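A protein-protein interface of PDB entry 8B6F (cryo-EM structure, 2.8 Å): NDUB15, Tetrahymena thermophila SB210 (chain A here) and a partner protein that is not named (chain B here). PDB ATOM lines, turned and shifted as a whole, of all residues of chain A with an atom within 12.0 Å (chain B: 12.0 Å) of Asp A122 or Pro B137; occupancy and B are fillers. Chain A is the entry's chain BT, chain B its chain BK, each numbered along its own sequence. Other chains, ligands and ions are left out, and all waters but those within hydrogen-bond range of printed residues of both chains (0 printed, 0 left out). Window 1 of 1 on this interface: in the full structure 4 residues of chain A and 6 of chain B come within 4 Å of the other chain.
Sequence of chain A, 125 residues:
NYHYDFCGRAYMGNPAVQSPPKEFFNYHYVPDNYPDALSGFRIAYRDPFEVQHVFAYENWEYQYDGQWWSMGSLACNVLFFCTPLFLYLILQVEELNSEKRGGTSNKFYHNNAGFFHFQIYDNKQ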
ATOM      1  N   GLY A 114      17.391  21.552 -29.838  1.00  0.00           N
ATOM      2  CA  GLY A 114      17.511  22.417 -28.686  1.00  0.00           C
ATOM      3  C   GLY A 114      18.934  22.642 -28.236  1.00  0.00           C
ATOM      4  O   GLY A 114      19.147  23.225 -27.168  1.00  0.00           O
ATOM      5  N   PHE A 115      19.914  22.198 -29.020  1.00  0.00           N
ATOM      6  CA  PHE A 115      21.324  22.349 -28.678  1.00  0.00           C
ATOM      7  C   PHE A 115      21.792  23.730 -29.118  1.00  0.00           C
ATOM      8  O   PHE A 115      21.878  24.014 -30.316  1.00  0.00           O
ATOM      9  CB  PHE A 115      22.153  21.255 -29.346  1.00  0.00           C
ATOM     10  CG  PHE A 115      21.878  19.875 -28.822  1.00  0.00           C
ATOM     11  CD1 PHE A 115      21.857  19.626 -27.461  1.00  0.00           C
ATOM     12  CD2 PHE A 115      21.639  18.826 -29.692  1.00  0.00           C
ATOM     13  CE1 PHE A 115      21.605  18.360 -26.977  1.00  0.00           C
ATOM     14  CE2 PHE A 115      21.385  17.557 -29.215  1.00  0.00           C
ATOM     15  CZ  PHE A 115      21.370  17.323 -27.856  1.00  0.00           C
ATOM     16  N   PHE A 116      22.095  24.588 -28.150  1.00  0.00           N
ATOM     17  CA  PHE A 116      22.463  25.961 -28.446  1.00  0.00           C
ATOM     18  C   PHE A 116      23.850  26.025 -29.081  1.00  0.00           C
ATOM     19  O   PHE A 116      24.655  25.095 -28.986  1.00  0.00           O
ATOM     20  CB  PHE A 116      22.424  26.806 -27.174  1.00  0.00           C
ATOM     21  CG  PHE A 116      21.071  26.855 -26.527  1.00  0.00           C
ATOM     22  CD1 PHE A 116      19.939  27.143 -27.273  1.00  0.00           C
ATOM     23  CD2 PHE A 116      20.926  26.594 -25.176  1.00  0.00           C
ATOM     24  CE1 PHE A 116      18.693  27.179 -26.683  1.00  0.00           C
ATOM     25  CE2 PHE A 116      19.683  26.629 -24.580  1.00  0.00           C
ATOM     26  CZ  PHE A 116      18.564  26.922 -25.335  1.00  0.00           C
ATOM     27  N   PHE A 118      27.408  26.250 -29.759  1.00  0.00           N
ATOM     28  CA  PHE A 118      28.647  26.089 -29.002  1.00  0.00           C
ATOM     29  C   PHE A 118      28.397  26.172 -27.497  1.00  0.00           C
ATOM     30  O   PHE A 118      29.099  26.870 -26.763  1.00  0.00           O
ATOM     31  CB  PHE A 118      29.690  27.121 -29.435  1.00  0.00           C
ATOM     32  CG  PHE A 118      30.455  26.728 -30.663  1.00  0.00           C
ATOM     33  CD1 PHE A 118      31.454  25.770 -30.593  1.00  0.00           C
ATOM     34  CD2 PHE A 118      30.195  27.330 -31.880  1.00  0.00           C
ATOM     35  CE1 PHE A 118      32.167  25.410 -31.719  1.00  0.00           C
ATOM     36  CE2 PHE A 118      30.904  26.975 -33.011  1.00  0.00           C
ATOM     37  CZ  PHE A 118      31.892  26.013 -32.930  1.00  0.00           C
ATOM     38  N   GLN A 119      27.382  25.453 -27.034  1.00  0.00           N
ATOM     39  CA  GLN A 119      27.108  25.384 -25.606  1.00  0.00           C
ATOM     40  C   GLN A 119      27.921  24.266 -24.966  1.00  0.00           C
ATOM     41  O   GLN A 119      28.270  23.274 -25.610  1.00  0.00           O
ATOM     42  CB  GLN A 119      25.620  25.155 -25.339  1.00  0.00           C
ATOM     43  CG  GLN A 119      25.018  26.161 -24.368  1.00  0.00           C
ATOM     44  CD  GLN A 119      23.894  25.588 -23.537  1.00  0.00           C
ATOM     45  OE1 GLN A 119      23.545  24.418 -23.661  1.00  0.00           O
ATOM     46  NE2 GLN A 119      23.321  26.418 -22.673  1.00  0.00           N
ATOM     47  N   ILE A 120      28.218  24.440 -23.684  1.00  0.00           N
ATOM     48  CA  ILE A 120      28.966  23.456 -22.910  1.00  0.00           C
ATOM     49  C   ILE A 120      27.966  22.473 -22.315  1.00  0.00           C
ATOM     50  O   ILE A 120      27.163  22.837 -21.454  1.00  0.00           O
ATOM     51  CB  ILE A 120      29.807  24.125 -21.816  1.00  0.00           C
ATOM     52  CG1 ILE A 120      30.759  25.163 -22.424  1.00  0.00           C
ATOM     53  CG2 ILE A 120      30.587  23.084 -21.027  1.00  0.00           C
ATOM     54  CD1 ILE A 120      31.765  24.598 -23.404  1.00  0.00           C
ATOM     55  N   TYR A 121      28.011  21.224 -22.771  1.00  0.00           N
ATOM     56  CA  TYR A 121      27.150  20.164 -22.256  1.00  0.00           C
ATOM     57  C   TYR A 121      28.010  19.180 -21.477  1.00  0.00           C
ATOM     58  O   TYR A 121      28.805  18.439 -22.063  1.00  0.00           O
ATOM     59  CB  TYR A 121      26.401  19.465 -23.389  1.00  0.00           C
ATOM     60  CG  TYR A 121      25.281  20.301 -23.950  1.00  0.00           C
ATOM     61  CD1 TYR A 121      24.081  20.429 -23.268  1.00  0.00           C
ATOM     62  CD2 TYR A 121      25.426  20.972 -25.155  1.00  0.00           C
ATOM     63  CE1 TYR A 121      23.057  21.196 -23.768  1.00  0.00           C
ATOM     64  CE2 TYR A 121      24.406  21.743 -25.664  1.00  0.00           C
ATOM     65  CZ  TYR A 121      23.224  21.851 -24.965  1.00  0.00           C
ATOM     66  OH  TYR A 121      22.203  22.619 -25.466  1.00  0.00           O
ATOM     67  N   ASP A 122      27.839  19.172 -20.158  1.00  0.00           N
ATOM     68  CA  ASP A 122      28.637  18.338 -19.274  1.00  0.00           C
ATOM     69  C   ASP A 122      27.744  17.743 -18.199  1.00  0.00           C
ATOM     70  O   ASP A 122      26.633  18.213 -17.949  1.00  0.00           O
ATOM     71  CB  ASP A 122      29.768  19.132 -18.613  1.00  0.00           C
ATOM     72  CG  ASP A 122      30.739  19.703 -19.615  1.00  0.00           C
ATOM     73  OD1 ASP A 122      30.953  19.066 -20.668  1.00  0.00           O
ATOM     74  OD2 ASP A 122      31.290  20.790 -19.351  1.00  0.00           O
ATOM     75  N   ASN A 123      28.254  16.696 -17.562  1.00  0.00           N
ATOM     76  CA  ASN A 123      27.597  16.049 -16.442  1.00  0.00           C
ATOM     77  C   ASN A 123      28.555  16.028 -15.260  1.00  0.00           C
ATOM     78  O   ASN A 123      29.774  16.117 -15.425  1.00  0.00           O
ATOM     79  CB  ASN A 123      27.157  14.625 -16.798  1.00  0.00           C
ATOM     80  CG  ASN A 123      26.398  14.565 -18.105  1.00  0.00           C
ATOM     81  OD1 ASN A 123      25.187  14.771 -18.144  1.00  0.00           O
ATOM     82  ND2 ASN A 123      27.110  14.281 -19.188  1.00  0.00           N
ATOM     83  N   LYS A 124      27.996  15.921 -14.060  1.00  0.00           N
ATOM     84  CA  LYS A 124      28.784  15.913 -12.840  1.00  0.00           C
ATOM     85  C   LYS A 124      28.674  14.560 -12.148  1.00  0.00           C
ATOM     86  O   LYS A 124      27.635  13.898 -12.199  1.00  0.00           O
ATOM     87  CB  LYS A 124      28.334  17.028 -11.892  1.00  0.00           C
ATOM     88  CG  LYS A 124      26.995  16.772 -11.219  1.00  0.00           C
ATOM     89  CD  LYS A 124      26.539  17.985 -10.427  1.00  0.00           C
ATOM     90  CE  LYS A 124      25.276  17.688  -9.635  1.00  0.00           C
ATOM     91  NZ  LYS A 124      25.550  16.859  -8.428  1.00  0.00           N
ATOM     92  N   GLN A 125      29.762  14.159 -11.499  1.00  0.00           N
ATOM     93  CA  GLN A 125      29.793  12.913 -10.745  1.00  0.00           C
ATOM     94  C   GLN A 125      28.778  12.940  -9.609  1.00  0.00           C
ATOM     95  O   GLN A 125      28.884  13.750  -8.689  1.00  0.00           O
ATOM     96  CB  GLN A 125      31.197  12.659 -10.194  1.00  0.00           C
ATOM     97  CG  GLN A 125      32.181  12.161 -11.240  1.00  0.00           C
ATOM     98  CD  GLN A 125      33.609  12.138 -10.740  1.00  0.00           C
ATOM     99  OE1 GLN A 125      33.940  12.769  -9.737  1.00  0.00           O
ATOM    100  NE2 GLN A 125      34.467  11.400 -11.437  1.00  0.00           N
ATOM    101  N   GLU B 130      21.171  14.263   0.523  1.00  0.00           N
ATOM    102  CA  GLU B 130      21.192  14.736  -0.856  1.00  0.00           C
ATOM    103  C   GLU B 130      20.695  16.171  -0.967  1.00  0.00           C
ATOM    104  O   GLU B 130      21.169  16.922  -1.826  1.00  0.00           O
ATOM    105  CB  GLU B 130      20.340  13.821  -1.735  1.00  0.00           C
ATOM    106  CG  GLU B 130      20.287  14.235  -3.202  1.00  0.00           C
ATOM    107  CD  GLU B 130      19.254  13.456  -3.992  1.00  0.00           C
ATOM    108  OE1 GLU B 130      18.389  12.810  -3.367  1.00  0.00           O
ATOM    109  OE2 GLU B 130      19.308  13.490  -5.239  1.00  0.00           O
ATOM    110  N   GLY B 133      23.171  18.987  -1.585  1.00  0.00           N
ATOM    111  CA  GLY B 133      23.774  19.131  -2.891  1.00  0.00           C
ATOM    112  C   GLY B 133      22.800  19.673  -3.920  1.00  0.00           C
ATOM    113  O   GLY B 133      21.630  19.936  -3.647  1.00  0.00           O
ATOM    114  N   ILE B 134      23.310  19.847  -5.134  1.00  0.00           N
ATOM    115  CA  ILE B 134      22.521  20.359  -6.245  1.00  0.00           C
ATOM    116  C   ILE B 134      22.206  19.207  -7.192  1.00  0.00           C
ATOM    117  O   ILE B 134      22.892  18.182  -7.219  1.00  0.00           O
ATOM    118  CB  ILE B 134      23.243  21.502  -6.988  1.00  0.00           C
ATOM    119  CG1 ILE B 134      24.456  20.959  -7.754  1.00  0.00           C
ATOM    120  CG2 ILE B 134      23.665  22.577  -5.995  1.00  0.00           C
ATOM    121  CD1 ILE B 134      25.266  22.011  -8.484  1.00  0.00           C
ATOM    122  N   THR B 135      21.149  19.386  -7.978  1.00  0.00           N
ATOM    123  CA  THR B 135      20.734  18.416  -8.991  1.00  0.00           C
ATOM    124  C   THR B 135      20.998  19.033 -10.361  1.00  0.00           C
ATOM    125  O   THR B 135      20.136  19.696 -10.937  1.00  0.00           O
ATOM    126  CB  THR B 135      19.268  18.023  -8.834  1.00  0.00           C
ATOM    127  OG1 THR B 135      18.453  19.199  -8.753  1.00  0.00           O
ATOM    128  CG2 THR B 135      19.070  17.153  -7.604  1.00  0.00           C
ATOM    129  N   ALA B 136      22.199  18.810 -10.874  1.00  0.00           N
ATOM    130  CA  ALA B 136      22.553  19.350 -12.172  1.00  0.00           C
ATOM    131  C   ALA B 136      21.891  18.533 -13.277  1.00  0.00           C
ATOM    132  O   ALA B 136      21.647  17.336 -13.112  1.00  0.00           O
ATOM    133  CB  ALA B 136      24.065  19.343 -12.360  1.00  0.00           C
ATOM    134  N   PRO B 137      21.585  19.154 -14.413  1.00  0.00           N
ATOM    135  CA  PRO B 137      20.985  18.397 -15.514  1.00  0.00           C
ATOM    136  C   PRO B 137      21.960  17.382 -16.087  1.00  0.00           C
ATOM    137  O   PRO B 137      23.177  17.579 -16.080  1.00  0.00           O
ATOM    138  CB  PRO B 137      20.637  19.479 -16.542  1.00  0.00           C
ATOM    139  CG  PRO B 137      21.587  20.583 -16.258  1.00  0.00           C
ATOM    140  CD  PRO B 137      21.818  20.563 -14.776  1.00  0.00           C
ATOM    141  N   LYS B 138      21.405  16.280 -16.583  1.00  0.00           N
ATOM    142  CA  LYS B 138      22.181  15.245 -17.263  1.00  0.00           C
ATOM    143  C   LYS B 138      22.064  15.498 -18.761  1.00  0.00           C
ATOM    144  O   LYS B 138      21.040  15.197 -19.377  1.00  0.00           O
ATOM    145  CB  LYS B 138      21.690  13.852 -16.890  1.00  0.00           C
ATOM    146  CG  LYS B 138      22.012  13.445 -15.463  1.00  0.00           C
ATOM    147  CD  LYS B 138      21.699  11.978 -15.236  1.00  0.00           C
ATOM    148  CE  LYS B 138      21.912  11.577 -13.787  1.00  0.00           C
ATOM    149  NZ  LYS B 138      23.335  11.717 -13.373  1.00  0.00           N
ATOM    150  N   ASN B 139      23.118  16.057 -19.344  1.00  0.00           N
ATOM    151  CA  ASN B 139      23.122  16.389 -20.757  1.00  0.00           C
ATOM    152  C   ASN B 139      23.563  15.187 -21.581  1.00  0.00           C
ATOM    153  O   ASN B 139      24.348  14.352 -21.126  1.00  0.00           O
ATOM    154  CB  ASN B 139      24.048  17.575 -21.030  1.00  0.00           C
ATOM    155  CG  ASN B 139      23.733  18.771 -20.156  1.00  0.00           C
ATOM    156  OD1 ASN B 139      22.769  19.495 -20.398  1.00  0.00           O
ATOM    157  ND2 ASN B 139      24.552  18.989 -19.136  1.00  0.00           N
ATOM    158  N   LEU B 140      23.041  15.104 -22.803  1.00  0.00           N
ATOM    159  CA  LEU B 140      23.375  14.023 -23.727  1.00  0.00           C
ATOM    160  C   LEU B 140      23.059  12.665 -23.098  1.00  0.00           C
ATOM    161  O   LEU B 140      23.935  11.831 -22.865  1.00  0.00           O
ATOM    162  CB  LEU B 140      24.841  14.111 -24.163  1.00  0.00           C
ATOM    163  CG  LEU B 140      25.186  15.191 -25.197  1.00  0.00           C
ATOM    164  CD1 LEU B 140      24.784  16.577 -24.729  1.00  0.00           C
ATOM    165  CD2 LEU B 140      26.667  15.163 -25.524  1.00  0.00           C
ATOM    166  N   SER B 141      21.776  12.465 -22.818  1.00  0.00           N
ATOM    167  CA  SER B 141      21.315  11.223 -22.223  1.00  0.00           C
ATOM    168  C   SER B 141      21.316  10.109 -23.267  1.00  0.00           C
ATOM    169  O   SER B 141      21.633  10.315 -24.441  1.00  0.00           O
ATOM    170  CB  SER B 141      19.920  11.409 -21.630  1.00  0.00           C
ATOM    171  OG  SER B 141      19.423  10.194 -21.097  1.00  0.00           O
ATOM    172  N   PHE B 142      20.958   8.904 -22.824  1.00  0.00           N
ATOM    173  CA  PHE B 142      20.897   7.741 -23.693  1.00  0.00           C
ATOM    174  C   PHE B 142      19.506   7.144 -23.828  1.00  0.00           C
ATOM    175  O   PHE B 142      19.243   6.467 -24.826  1.00  0.00           O
ATOM    176  CB  PHE B 142      21.850   6.645 -23.190  1.00  0.00           C
ATOM    177  CG  PHE B 142      21.550   6.178 -21.796  1.00  0.00           C
ATOM    178  CD1 PHE B 142      20.636   5.163 -21.574  1.00  0.00           C
ATOM    179  CD2 PHE B 142      22.186   6.750 -20.708  1.00  0.00           C
ATOM    180  CE1 PHE B 142      20.359   4.728 -20.295  1.00  0.00           C
ATOM    181  CE2 PHE B 142      21.913   6.320 -19.424  1.00  0.00           C
ATOM    182  CZ  PHE B 142      20.998   5.308 -19.219  1.00  0.00           C
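The backbone carbonyl oxygen of Ile B134 lies within hydrogen-bond range of the side-chain amino group of Lys A124, 3.2 Å away. The backbone carbonyl oxygen (O) of Asp A122 sits at hydrogen-bond distance from the side-chain amide nitrogen (ND2) of Asn B139. The backbone NH of Asn B139 lies within hydrogen-bond range of the side-chain amide oxygen of Asn A123 (2.7 Å).
N of Phe A116 sits at hydrogen-bond distance from OH of Tyr A121, at 3.3 Å. OE1 of Gln A119 sits at hydrogen-bond distance from OH of Tyr A121 (2.9 Å).
Among the printed residues, merely in contact across the chains: Tyr A121 with Asn B139 (3.3 Å), Tyr A121 with Leu B140 (3.6 Å), Asp A122 with Pro B137 (3.98 Å), Asn A123 with Lys B138 (3.2 Å) and Lys A124 with Ala B136 (3.4 Å).
Printed residues of chain B within 4 Å of Asp A122: Pro B137 and Asn B139. Printed residues of chain A within 4 Å of Pro B137: Asp A122. No residue of chain B comes within 4 Å of Ile A120. Asn A123 touches two residues of chain B. Lys A124 touches two residues of chain B. No residue of chain A comes within 4 Å of Thr B135. Printed residues of chain A within 4 Å of Ala B136: Lys A124. Of chain A, only Asn A123 (3.2 Å) comes within 4 Å of Lys B138. Asn B139 touches just these residues of chain A: Tyr A121 (3.3 Å), Asp A122 (2.5 Å) and Asn A123 (2.7 Å). Of the printed residues of chain A, Ile B134 touches Lys A124. Printed residues of chain B within 4 Å of Tyr A121: Asn B139 and Leu B140. Phe A115 touches none of the printed residues of chain B. The nearest residue of chain B that does not touch Asp A122 is Lys B138 (5.4 Å). The nearest printed residue of chain A that does not touch Leu B140 is Phe A115 (4.3 Å).
Hydrophobic or aromatic side chains of chain B that line the printed part of chain A: Ile B134, Ala B136 and Leu B140. Printed residues of chain A that touch a printed residue of chain B: Tyr A121, Asp A122, Asn A123 and Lys A124. Among the printed residues, no Asp or Glu carboxylate lies within 4 Å of a Lys or Arg side-chain nitrogen of the other chain.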
